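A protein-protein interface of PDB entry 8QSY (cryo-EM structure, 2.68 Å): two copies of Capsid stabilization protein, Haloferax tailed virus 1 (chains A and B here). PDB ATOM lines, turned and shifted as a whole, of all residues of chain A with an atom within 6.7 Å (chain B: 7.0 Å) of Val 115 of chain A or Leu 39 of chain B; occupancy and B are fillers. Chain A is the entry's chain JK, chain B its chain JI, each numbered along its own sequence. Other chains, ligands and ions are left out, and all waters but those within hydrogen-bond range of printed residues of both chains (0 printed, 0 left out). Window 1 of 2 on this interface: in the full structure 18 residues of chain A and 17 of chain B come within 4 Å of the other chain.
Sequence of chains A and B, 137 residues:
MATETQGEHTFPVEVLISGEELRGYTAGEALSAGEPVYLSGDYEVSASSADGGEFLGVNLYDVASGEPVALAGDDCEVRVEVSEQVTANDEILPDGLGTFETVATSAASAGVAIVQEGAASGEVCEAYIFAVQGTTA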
ATOM      1  N   VAL A  82      -2.150  12.505  -3.454  1.00  0.00           N
ATOM      2  CA  VAL A  82      -0.979  12.953  -4.194  1.00  0.00           C
ATOM      3  C   VAL A  82      -0.555  11.878  -5.190  1.00  0.00           C
ATOM      4  O   VAL A  82      -0.568  10.694  -4.873  1.00  0.00           O
ATOM      5  CB  VAL A  82       0.176  13.341  -3.250  1.00  0.00           C
ATOM      6  CG1 VAL A  82      -0.103  14.686  -2.614  1.00  0.00           C
ATOM      7  CG2 VAL A  82       0.453  12.289  -2.179  1.00  0.00           C
ATOM      8  N   VAL A  86       5.358  12.480  -0.894  1.00  0.00           N
ATOM      9  CA  VAL A  86       5.490  13.819  -0.319  1.00  0.00           C
ATOM     10  C   VAL A  86       5.749  13.741   1.185  1.00  0.00           C
ATOM     11  O   VAL A  86       5.382  12.778   1.854  1.00  0.00           O
ATOM     12  CB  VAL A  86       4.267  14.718  -0.595  1.00  0.00           C
ATOM     13  CG1 VAL A  86       3.958  14.860  -2.074  1.00  0.00           C
ATOM     14  CG2 VAL A  86       3.018  14.282   0.163  1.00  0.00           C
ATOM     15  N   THR A  87       6.325  14.825   1.716  1.00  0.00           N
ATOM     16  CA  THR A  87       6.780  14.939   3.094  1.00  0.00           C
ATOM     17  C   THR A  87       6.270  16.246   3.696  1.00  0.00           C
ATOM     18  O   THR A  87       5.925  17.180   2.976  1.00  0.00           O
ATOM     19  CB  THR A  87       8.315  14.914   3.156  1.00  0.00           C
ATOM     20  OG1 THR A  87       8.853  16.038   2.460  1.00  0.00           O
ATOM     21  CG2 THR A  87       8.913  13.663   2.557  1.00  0.00           C
ATOM     22  N   ALA A  88       6.228  16.325   5.031  1.00  0.00           N
ATOM     23  CA  ALA A  88       5.833  17.558   5.703  1.00  0.00           C
ATOM     24  C   ALA A  88       6.714  18.735   5.265  1.00  0.00           C
ATOM     25  O   ALA A  88       7.898  18.567   4.981  1.00  0.00           O
ATOM     26  CB  ALA A  88       5.862  17.354   7.195  1.00  0.00           C
ATOM     27  N   ASN A  89       6.107  19.931   5.171  1.00  0.00           N
ATOM     28  CA  ASN A  89       6.702  21.143   4.626  1.00  0.00           C
ATOM     29  C   ASN A  89       6.833  21.156   3.092  1.00  0.00           C
ATOM     30  O   ASN A  89       7.245  22.187   2.563  1.00  0.00           O
ATOM     31  CB  ASN A  89       8.025  21.524   5.307  1.00  0.00           C
ATOM     32  CG  ASN A  89       8.311  23.012   5.300  1.00  0.00           C
ATOM     33  OD1 ASN A  89       7.565  23.794   5.882  1.00  0.00           O
ATOM     34  ND2 ASN A  89       9.400  23.420   4.664  1.00  0.00           N
ATOM     35  N   ASP A  90       6.496  20.090   2.347  1.00  0.00           N
ATOM     36  CA  ASP A  90       6.471  20.216   0.891  1.00  0.00           C
ATOM     37  C   ASP A  90       5.325  21.127   0.452  1.00  0.00           C
ATOM     38  O   ASP A  90       4.187  20.958   0.888  1.00  0.00           O
ATOM     39  CB  ASP A  90       6.355  18.860   0.191  1.00  0.00           C
ATOM     40  CG  ASP A  90       7.612  18.014   0.281  1.00  0.00           C
ATOM     41  OD1 ASP A  90       8.706  18.612   0.407  1.00  0.00           O
ATOM     42  OD2 ASP A  90       7.495  16.764   0.196  1.00  0.00           O
ATOM     43  N   GLU A  91       5.624  22.084  -0.433  1.00  0.00           N
ATOM     44  CA  GLU A  91       4.553  22.754  -1.152  1.00  0.00           C
ATOM     45  C   GLU A  91       4.076  21.869  -2.300  1.00  0.00           C
ATOM     46  O   GLU A  91       4.868  21.283  -3.046  1.00  0.00           O
ATOM     47  CB  GLU A  91       4.970  24.128  -1.657  1.00  0.00           C
ATOM     48  CG  GLU A  91       5.103  25.132  -0.536  1.00  0.00           C
ATOM     49  CD  GLU A  91       5.231  26.587  -0.961  1.00  0.00           C
ATOM     50  OE1 GLU A  91       4.966  26.896  -2.149  1.00  0.00           O
ATOM     51  OE2 GLU A  91       5.578  27.422  -0.099  1.00  0.00           O
ATOM     52  N   ILE A  92       2.752  21.821  -2.454  1.00  0.00           N
ATOM     53  CA  ILE A  92       2.091  21.009  -3.455  1.00  0.00           C
ATOM     54  C   ILE A  92       1.162  21.879  -4.295  1.00  0.00           C
ATOM     55  O   ILE A  92       0.785  22.991  -3.924  1.00  0.00           O
ATOM     56  CB  ILE A  92       1.376  19.787  -2.835  1.00  0.00           C
ATOM     57  CG1 ILE A  92       0.331  20.183  -1.783  1.00  0.00           C
ATOM     58  CG2 ILE A  92       2.398  18.790  -2.302  1.00  0.00           C
ATOM     59  CD1 ILE A  92      -0.667  19.094  -1.443  1.00  0.00           C
ATOM     60  N   THR A 102       4.150  17.725  -5.911  1.00  0.00           N
ATOM     61  CA  THR A 102       4.941  18.811  -5.349  1.00  0.00           C
ATOM     62  C   THR A 102       5.254  19.894  -6.375  1.00  0.00           C
ATOM     63  O   THR A 102       5.390  19.644  -7.574  1.00  0.00           O
ATOM     64  CB  THR A 102       6.271  18.348  -4.752  1.00  0.00           C
ATOM     65  OG1 THR A 102       7.093  17.808  -5.782  1.00  0.00           O
ATOM     66  CG2 THR A 102       6.088  17.335  -3.649  1.00  0.00           C
ATOM     67  N   ALA A 113      -0.860  24.639  -1.521  1.00  0.00           N
ATOM     68  CA  ALA A 113      -1.062  23.991  -0.235  1.00  0.00           C
ATOM     69  C   ALA A 113       0.271  23.438   0.268  1.00  0.00           C
ATOM     70  O   ALA A 113       1.177  23.154  -0.519  1.00  0.00           O
ATOM     71  CB  ALA A 113      -2.132  22.929  -0.356  1.00  0.00           C
ATOM     72  N   ILE A 114       0.398  23.325   1.591  1.00  0.00           N
ATOM     73  CA  ILE A 114       1.594  22.815   2.235  1.00  0.00           C
ATOM     74  C   ILE A 114       1.245  21.501   2.934  1.00  0.00           C
ATOM     75  O   ILE A 114       0.225  21.412   3.615  1.00  0.00           O
ATOM     76  CB  ILE A 114       2.188  23.882   3.178  1.00  0.00           C
ATOM     77  CG1 ILE A 114       3.585  23.482   3.648  1.00  0.00           C
ATOM     78  CG2 ILE A 114       1.264  24.207   4.350  1.00  0.00           C
ATOM     79  CD1 ILE A 114       4.313  24.585   4.373  1.00  0.00           C
ATOM     80  N   VAL A 115       2.078  20.476   2.738  1.00  0.00           N
ATOM     81  CA  VAL A 115       1.840  19.162   3.315  1.00  0.00           C
ATOM     82  C   VAL A 115       2.135  19.211   4.809  1.00  0.00           C
ATOM     83  O   VAL A 115       3.234  19.576   5.219  1.00  0.00           O
ATOM     84  CB  VAL A 115       2.704  18.101   2.610  1.00  0.00           C
ATOM     85  CG1 VAL A 115       2.635  16.747   3.295  1.00  0.00           C
ATOM     86  CG2 VAL A 115       2.288  17.964   1.165  1.00  0.00           C
ATOM     87  N   GLN A 116       1.154  18.803   5.614  1.00  0.00           N
ATOM     88  CA  GLN A 116       1.318  18.674   7.054  1.00  0.00           C
ATOM     89  C   GLN A 116       1.629  17.230   7.456  1.00  0.00           C
ATOM     90  O   GLN A 116       2.239  16.994   8.495  1.00  0.00           O
ATOM     91  CB  GLN A 116       0.034  19.116   7.744  1.00  0.00           C
ATOM     92  CG  GLN A 116      -0.319  20.571   7.482  1.00  0.00           C
ATOM     93  CD  GLN A 116      -1.661  20.937   8.069  1.00  0.00           C
ATOM     94  OE1 GLN A 116      -2.596  20.136   8.115  1.00  0.00           O
ATOM     95  NE2 GLN A 116      -1.790  22.171   8.534  1.00  0.00           N
ATOM     96  N   GLU A 117       1.218  16.265   6.625  1.00  0.00           N
ATOM     97  CA  GLU A 117       1.314  14.841   6.919  1.00  0.00           C
ATOM     98  C   GLU A 117       1.650  14.114   5.618  1.00  0.00           C
ATOM     99  O   GLU A 117       0.846  14.119   4.691  1.00  0.00           O
ATOM    100  CB  GLU A 117      -0.025  14.393   7.512  1.00  0.00           C
ATOM    101  CG  GLU A 117       0.109  13.500   8.742  1.00  0.00           C
ATOM    102  CD  GLU A 117       0.489  12.052   8.486  1.00  0.00           C
ATOM    103  OE1 GLU A 117       0.079  11.504   7.443  1.00  0.00           O
ATOM    104  OE2 GLU A 117       1.188  11.468   9.341  1.00  0.00           O
ATOM    105  N   GLY A 118       2.866  13.551   5.527  1.00  0.00           N
ATOM    106  CA  GLY A 118       3.378  12.946   4.300  1.00  0.00           C
ATOM    107  C   GLY A 118       2.587  11.721   3.825  1.00  0.00           C
ATOM    108  O   GLY A 118       1.850  11.096   4.587  1.00  0.00           O
ATOM    109  N   ALA A 119       2.756  11.371   2.543  1.00  0.00           N
ATOM    110  CA  ALA A 119       2.070  10.238   1.934  1.00  0.00           C
ATOM    111  C   ALA A 119       2.899   9.671   0.779  1.00  0.00           C
ATOM    112  O   ALA A 119       3.683  10.386   0.161  1.00  0.00           O
ATOM    113  CB  ALA A 119       0.698  10.669   1.458  1.00  0.00           C
ATOM    114  N   CYS A 125      -2.459  12.406   1.583  1.00  0.00           N
ATOM    115  CA  CYS A 125      -1.775  13.290   2.514  1.00  0.00           C
ATOM    116  C   CYS A 125      -2.789  14.202   3.215  1.00  0.00           C
ATOM    117  O   CYS A 125      -3.942  14.305   2.798  1.00  0.00           O
ATOM    118  CB  CYS A 125      -0.719  14.098   1.764  1.00  0.00           C
ATOM    119  SG  CYS A 125      -1.423  15.500   0.856  1.00  0.00           S
ATOM    120  N   GLU A 126      -2.360  14.884   4.288  1.00  0.00           N
ATOM    121  CA  GLU A 126      -3.122  16.000   4.837  1.00  0.00           C
ATOM    122  C   GLU A 126      -2.340  17.291   4.604  1.00  0.00           C
ATOM    123  O   GLU A 126      -1.148  17.363   4.905  1.00  0.00           O
ATOM    124  CB  GLU A 126      -3.462  15.781   6.313  1.00  0.00           C
ATOM    125  CG  GLU A 126      -4.288  14.524   6.558  1.00  0.00           C
ATOM    126  CD  GLU A 126      -5.074  14.480   7.862  1.00  0.00           C
ATOM    127  OE1 GLU A 126      -4.709  15.210   8.808  1.00  0.00           O
ATOM    128  OE2 GLU A 126      -6.073  13.723   7.927  1.00  0.00           O
ATOM    129  N   ALA A 127      -3.023  18.313   4.071  1.00  0.00           N
ATOM    130  CA  ALA A 127      -2.380  19.544   3.626  1.00  0.00           C
ATOM    131  C   ALA A 127      -3.226  20.772   3.975  1.00  0.00           C
ATOM    132  O   ALA A 127      -4.448  20.693   4.059  1.00  0.00           O
ATOM    133  CB  ALA A 127      -2.128  19.463   2.140  1.00  0.00           C
ATOM    134  N   TYR A 128      -2.573  21.927   4.155  1.00  0.00           N
ATOM    135  CA  TYR A 128      -3.250  23.192   4.396  1.00  0.00           C
ATOM    136  C   TYR A 128      -3.187  24.058   3.139  1.00  0.00           C
ATOM    137  O   TYR A 128      -2.097  24.350   2.657  1.00  0.00           O
ATOM    138  CB  TYR A 128      -2.571  23.894   5.572  1.00  0.00           C
ATOM    139  CG  TYR A 128      -3.058  25.287   5.881  1.00  0.00           C
ATOM    140  CD1 TYR A 128      -4.347  25.502   6.360  1.00  0.00           C
ATOM    141  CD2 TYR A 128      -2.223  26.390   5.724  1.00  0.00           C
ATOM    142  CE1 TYR A 128      -4.794  26.781   6.669  1.00  0.00           C
ATOM    143  CE2 TYR A 128      -2.662  27.676   6.012  1.00  0.00           C
ATOM    144  CZ  TYR A 128      -3.954  27.870   6.485  1.00  0.00           C
ATOM    145  OH  TYR A 128      -4.396  29.127   6.797  1.00  0.00           O
ATOM    146  N   TYR B  25      -0.205  21.668  16.695  1.00  0.00           N
ATOM    147  CA  TYR B  25       0.913  20.870  16.199  1.00  0.00           C
ATOM    148  C   TYR B  25       1.646  20.259  17.391  1.00  0.00           C
ATOM    149  O   TYR B  25       1.369  20.614  18.527  1.00  0.00           O
ATOM    150  CB  TYR B  25       1.857  21.732  15.346  1.00  0.00           C
ATOM    151  CG  TYR B  25       1.140  22.257  14.134  1.00  0.00           C
ATOM    152  CD1 TYR B  25       1.050  21.492  12.977  1.00  0.00           C
ATOM    153  CD2 TYR B  25       0.453  23.466  14.195  1.00  0.00           C
ATOM    154  CE1 TYR B  25       0.251  21.903  11.920  1.00  0.00           C
ATOM    155  CE2 TYR B  25      -0.340  23.888  13.142  1.00  0.00           C
ATOM    156  CZ  TYR B  25      -0.449  23.098  12.009  1.00  0.00           C
ATOM    157  OH  TYR B  25      -1.242  23.478  10.970  1.00  0.00           O
ATOM    158  N   VAL B  37       7.765  29.475  13.474  1.00  0.00           N
ATOM    159  CA  VAL B  37       7.971  28.035  13.354  1.00  0.00           C
ATOM    160  C   VAL B  37       7.553  27.523  11.972  1.00  0.00           C
ATOM    161  O   VAL B  37       6.773  28.160  11.272  1.00  0.00           O
ATOM    162  CB  VAL B  37       7.245  27.267  14.476  1.00  0.00           C
ATOM    163  CG1 VAL B  37       7.700  27.713  15.853  1.00  0.00           C
ATOM    164  CG2 VAL B  37       5.729  27.358  14.381  1.00  0.00           C
ATOM    165  N   TYR B  38       8.055  26.337  11.601  1.00  0.00           N
ATOM    166  CA  TYR B  38       7.783  25.677  10.328  1.00  0.00           C
ATOM    167  C   TYR B  38       7.643  24.165  10.554  1.00  0.00           C
ATOM    168  O   TYR B  38       8.067  23.661  11.590  1.00  0.00           O
ATOM    169  CB  TYR B  38       8.926  25.965   9.347  1.00  0.00           C
ATOM    170  CG  TYR B  38      10.124  25.068   9.534  1.00  0.00           C
ATOM    171  CD1 TYR B  38      10.991  25.245  10.605  1.00  0.00           C
ATOM    172  CD2 TYR B  38      10.338  23.986   8.694  1.00  0.00           C
ATOM    173  CE1 TYR B  38      12.042  24.365  10.828  1.00  0.00           C
ATOM    174  CE2 TYR B  38      11.383  23.097   8.907  1.00  0.00           C
ATOM    175  CZ  TYR B  38      12.239  23.287   9.980  1.00  0.00           C
ATOM    176  OH  TYR B  38      13.282  22.425  10.180  1.00  0.00           O
ATOM    177  N   LEU B  39       7.093  23.431   9.572  1.00  0.00           N
ATOM    178  CA  LEU B  39       6.897  21.989   9.696  1.00  0.00           C
ATOM    179  C   LEU B  39       8.214  21.216   9.600  1.00  0.00           C
ATOM    180  O   LEU B  39       8.830  21.143   8.540  1.00  0.00           O
ATOM    181  CB  LEU B  39       5.900  21.519   8.636  1.00  0.00           C
ATOM    182  CG  LEU B  39       4.451  21.875   8.950  1.00  0.00           C
ATOM    183  CD1 LEU B  39       3.655  22.114   7.683  1.00  0.00           C
ATOM    184  CD2 LEU B  39       3.786  20.832   9.839  1.00  0.00           C
ATOM    185  N   SER B  40       8.623  20.596  10.715  1.00  0.00           N
ATOM    186  CA  SER B  40       9.808  19.754  10.806  1.00  0.00           C
ATOM    187  C   SER B  40       9.490  18.261  10.663  1.00  0.00           C
ATOM    188  O   SER B  40      10.410  17.458  10.503  1.00  0.00           O
ATOM    189  CB  SER B  40      10.560  20.051  12.076  1.00  0.00           C
ATOM    190  OG  SER B  40       9.676  20.060  13.197  1.00  0.00           O
ATOM    191  N   GLY B  41       8.201  17.889  10.721  1.00  0.00           N
ATOM    192  CA  GLY B  41       7.741  16.514  10.558  1.00  0.00           C
ATOM    193  C   GLY B  41       6.217  16.447  10.478  1.00  0.00           C
ATOM    194  O   GLY B  41       5.560  17.485  10.462  1.00  0.00           O
ATOM    195  N   ASP B  42       5.648  15.235  10.448  1.00  0.00           N
ATOM    196  CA  ASP B  42       4.202  15.068  10.334  1.00  0.00           C
ATOM    197  C   ASP B  42       3.487  15.708  11.527  1.00  0.00           C
ATOM    198  O   ASP B  42       3.622  15.238  12.654  1.00  0.00           O
ATOM    199  CB  ASP B  42       3.823  13.596  10.168  1.00  0.00           C
ATOM    200  CG  ASP B  42       4.299  12.958   8.872  1.00  0.00           C
ATOM    201  OD1 ASP B  42       4.379  13.669   7.845  1.00  0.00           O
ATOM    202  OD2 ASP B  42       4.581  11.741   8.897  1.00  0.00           O
ATOM    203  N   TYR B  43       2.715  16.780  11.265  1.00  0.00           N
ATOM    204  CA  TYR B  43       2.103  17.646  12.268  1.00  0.00           C
ATOM    205  C   TYR B  43       3.072  18.102  13.372  1.00  0.00           C
ATOM    206  O   TYR B  43       2.650  18.404  14.490  1.00  0.00           O
ATOM    207  CB  TYR B  43       0.809  17.023  12.795  1.00  0.00           C
ATOM    208  CG  TYR B  43      -0.373  17.170  11.872  1.00  0.00           C
ATOM    209  CD1 TYR B  43      -1.093  18.355  11.828  1.00  0.00           C
ATOM    210  CD2 TYR B  43      -0.781  16.135  11.041  1.00  0.00           C
ATOM    211  CE1 TYR B  43      -2.192  18.510  10.994  1.00  0.00           C
ATOM    212  CE2 TYR B  43      -1.876  16.275  10.196  1.00  0.00           C
ATOM    213  CZ  TYR B  43      -2.588  17.465  10.174  1.00  0.00           C
ATOM    214  OH  TYR B  43      -3.669  17.615   9.349  1.00  0.00           O
ATOM    215  N   GLU B  44       4.370  18.207  13.063  1.00  0.00           N
ATOM    216  CA  GLU B  44       5.382  18.651  14.016  1.00  0.00           C
ATOM    217  C   GLU B  44       6.043  19.932  13.510  1.00  0.00           C
ATOM    218  O   GLU B  44       6.421  20.005  12.343  1.00  0.00           O
ATOM    219  CB  GLU B  44       6.417  17.546  14.217  1.00  0.00           C
ATOM    220  CG  GLU B  44       7.533  17.920  15.174  1.00  0.00           C
ATOM    221  CD  GLU B  44       8.803  17.151  14.870  1.00  0.00           C
ATOM    222  OE1 GLU B  44       8.824  15.926  15.124  1.00  0.00           O
ATOM    223  OE2 GLU B  44       9.771  17.770  14.379  1.00  0.00           O
ATOM    224  N   VAL B  45       6.219  20.924  14.398  1.00  0.00           N
ATOM    225  CA  VAL B  45       6.804  22.215  14.050  1.00  0.00           C
ATOM    226  C   VAL B  45       8.036  22.530  14.905  1.00  0.00           C
ATOM    227  O   VAL B  45       8.086  22.201  16.087  1.00  0.00           O
ATOM    228  CB  VAL B  45       5.772  23.359  14.117  1.00  0.00           C
ATOM    229  CG1 VAL B  45       4.633  23.157  13.131  1.00  0.00           C
ATOM    230  CG2 VAL B  45       5.226  23.580  15.525  1.00  0.00           C
ATOM    231  N   SER B  46       9.012  23.227  14.300  1.00  0.00           N
ATOM    232  CA  SER B  46      10.271  23.636  14.917  1.00  0.00           C
ATOM    233  C   SER B  46      10.585  25.081  14.533  1.00  0.00           C
ATOM    234  O   SER B  46       9.969  25.616  13.619  1.00  0.00           O
ATOM    235  CB  SER B  46      11.380  22.724  14.480  1.00  0.00           C
ATOM    236  OG  SER B  46      11.175  21.411  14.968  1.00  0.00           O
ATOM    237  N   SER B  48      11.844  28.363  12.854  1.00  0.00           N
ATOM    238  CA  SER B  48      12.210  28.726  11.489  1.00  0.00           C
ATOM    239  C   SER B  48      13.676  29.148  11.364  1.00  0.00           C
ATOM    240  O   SER B  48      14.144  29.955  12.158  1.00  0.00           O
ATOM    241  CB  SER B  48      11.376  29.890  11.058  1.00  0.00           C
ATOM    242  OG  SER B  48      10.019  29.531  10.957  1.00  0.00           O
ATOM    243  N   GLU B  54      10.506  28.321   5.215  1.00  0.00           N
ATOM    244  CA  GLU B  54      10.302  27.710   6.523  1.00  0.00           C
ATOM    245  C   GLU B  54       9.449  28.623   7.404  1.00  0.00           C
ATOM    246  O   GLU B  54       9.954  29.243   8.337  1.00  0.00           O
ATOM    247  CB  GLU B  54      11.642  27.425   7.204  1.00  0.00           C
ATOM    248  CG  GLU B  54      12.384  26.240   6.627  1.00  0.00           C
ATOM    249  CD  GLU B  54      13.641  25.881   7.401  1.00  0.00           C
ATOM    250  OE1 GLU B  54      13.910  26.531   8.433  1.00  0.00           O
ATOM    251  OE2 GLU B  54      14.380  24.984   6.942  1.00  0.00           O
ATOM    252  N   PHE B  55       8.142  28.690   7.132  1.00  0.00           N
ATOM    253  CA  PHE B  55       7.238  29.389   8.026  1.00  0.00           C
ATOM    254  C   PHE B  55       5.809  28.876   7.872  1.00  0.00           C
ATOM    255  O   PHE B  55       5.249  28.931   6.780  1.00  0.00           O
ATOM    256  CB  PHE B  55       7.280  30.893   7.754  1.00  0.00           C
ATOM    257  CG  PHE B  55       6.342  31.682   8.630  1.00  0.00           C
ATOM    258  CD1 PHE B  55       6.698  32.024   9.929  1.00  0.00           C
ATOM    259  CD2 PHE B  55       5.090  32.067   8.164  1.00  0.00           C
ATOM    260  CE1 PHE B  55       5.829  32.747  10.735  1.00  0.00           C
ATOM    261  CE2 PHE B  55       4.226  32.804   8.963  1.00  0.00           C
ATOM    262  CZ  PHE B  55       4.600  33.147  10.246  1.00  0.00           C
ATOM    263  N   LEU B  56       5.204  28.436   8.988  1.00  0.00           N
ATOM    264  CA  LEU B  56       3.793  28.097   9.041  1.00  0.00           C
ATOM    265  C   LEU B  56       3.002  29.080   9.914  1.00  0.00           C
ATOM    266  O   LEU B  56       1.838  29.359   9.622  1.00  0.00           O
ATOM    267  CB  LEU B  56       3.654  26.659   9.541  1.00  0.00           C
ATOM    268  CG  LEU B  56       2.243  26.087   9.478  1.00  0.00           C
ATOM    269  CD1 LEU B  56       1.803  25.865   8.036  1.00  0.00           C
ATOM    270  CD2 LEU B  56       2.174  24.795  10.260  1.00  0.00           C
ATOM    271  N   GLN B 133       5.207  29.682   4.052  1.00  0.00           N
ATOM    272  CA  GLN B 133       6.235  29.286   3.105  1.00  0.00           C
ATOM    273  C   GLN B 133       6.733  27.887   3.439  1.00  0.00           C
ATOM    274  O   GLN B 133       7.160  27.624   4.564  1.00  0.00           O
ATOM    275  CB  GLN B 133       7.400  30.274   3.138  1.00  0.00           C
ATOM    276  CG  GLN B 133       7.028  31.654   2.616  1.00  0.00           C
ATOM    277  CD  GLN B 133       8.192  32.614   2.588  1.00  0.00           C
ATOM    278  OE1 GLN B 133       9.323  32.267   2.921  1.00  0.00           O
ATOM    279  NE2 GLN B 133       7.912  33.852   2.208  1.00  0.00           N
ATOM    280  N   THR B 135       8.736  24.114   1.436  1.00  0.00           N
ATOM    281  CA  THR B 135       9.756  23.628   0.524  1.00  0.00           C
ATOM    282  C   THR B 135       9.221  23.663  -0.907  1.00  0.00           C
ATOM    283  O   THR B 135       8.338  22.882  -1.254  1.00  0.00           O
ATOM    284  CB  THR B 135      10.153  22.185   0.867  1.00  0.00           C
ATOM    285  OG1 THR B 135       9.969  21.924   2.259  1.00  0.00           O
ATOM    286  CG2 THR B 135      11.573  21.858   0.465  1.00  0.00           C
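No position is printed for both chains. Of the 17 pairs that touch across the chains among the printed residues, none has its exchanged pair printed and touching as well.
The backbone NH (N) of Tyr 38 of chain B lies within hydrogen-bond range of the backbone carbonyl oxygen (O) of Ser 46 of chain B, 2.9 Å away. The backbone NH (N) of Glu 54 of chain B lies within hydrogen-bond range of the backbone carbonyl oxygen (O) of Gln 133 of chain B, 3.5 Å away. OD2 of Asp 90 of chain A sits at hydrogen-bond distance from N of Thr 87 of chain A, 2.7 Å away. N of Asn 89 of chain A lies within hydrogen-bond range of O of Val 115 of chain A (2.9 Å). The backbone carbonyl oxygen (O) of Asp 90 of chain A is in hydrogen-bond range of the backbone NH (N) of Val 115 of chain A (2.8 Å). The backbone carbonyl oxygen of Glu 126 of chain A sits at hydrogen-bond distance from the backbone NH of Gln 116 of chain A (2.8 Å).
O of Gly 41 of chain B touches CB of Ala 88 of chain A (3.3 Å). Asp 42 of chain B touches Ala 88 of chain A. Asn 89 of chain A touches Tyr 38 of chain B (OD1 to CD2, 3.95 Å). CB of Asn 89 of chain A touches O of Leu 39 of chain B, at 3.4 Å. Thr 135 of chain B touches Asp 90 of chain A (O to C, 3.9 Å). Glu 91 of chain A touches Gln 133 of chain B (OE2 to C, 3.8 Å). O of Val 115 of chain A touches CD1 of Leu 39 of chain B (3.6 Å). Gly 41 of chain B touches Gln 116 of chain A. Asp 42 of chain B touches Gln 116 of chain A (CA to O, 3.3 Å). Glu 117 of chain A touches Tyr 43 of chain B.
Hydrophobic or aromatic side chains of chain B that line the printed part of chain A: Tyr 25, Tyr 38, Leu 39 and Tyr 43. Hydrophobic or aromatic side chains of chain A within 4 Å of the printed part of chain B: Ala 88. Along chain A the printed residues that touch a printed residue of chain B span positions 88 to 126.
Of the printed residues of chain B, Val 115 of chain A touches Leu 39 (3.6 Å). Leu 39 of chain B touches just these residues of chain A: Asn 89 and Val 115. Printed residues of chain A within 4 Å of Tyr 25 of chain B: Gln 116 (2.8 Å). Of the printed residues of chain A, Gly 41 of chain B touches Ala 88 and Gln 116. Of the printed residues of chain B, Gln 116 of chain A touches Tyr 25 (2.8 Å), Gly 41 (3.9 Å), Asp 42 (3.3 Å) and Tyr 43 (2.8 Å). Of the printed residues of chain B, Ala 88 of chain A touches Gly 41 and Asp 42. Val 86 of chain A touches none of the printed residues of chain B. Ala 127 of chain A touches none of the printed residues of chain B. The nearest residue of chain B that does not touch Val 115 of chain A is Asp 42 of chain B (5.8 Å). The nearest printed residue of chain B that does not touch Asn 89 of chain A is Gln 133 of chain B (4.1 Å).
The side-chain hydroxyl of Tyr 25 of chain B is in hydrogen-bond range of the side-chain amide nitrogen of Gln 116 of chain A, at 2.8 Å. OD1 of Asp 42 of chain B lies within hydrogen-bond range of N of Gly 118 of chain A (2.8 Å). N of Tyr 43 of chain B sits at hydrogen-bond distance from O of Gln 116 of chain A (2.8 Å). OH of Tyr 43 of chain B sits at hydrogen-bond distance from OE1 of Glu 126 of chain A (2.7 Å). O of Asn 89 of chain A sits at hydrogen-bond distance from N of Thr 135 of chain B, at 2.7 Å. The backbone carbonyl oxygen of Thr 135 of chain B lies within hydrogen-bond range of the backbone NH of Glu 91 of chain A (2.9 Å). The side-chain carboxylate of Glu 117 of chain A lies close to the side-chain carboxylate of Asp 42 of chain B, 3.4 Å away.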
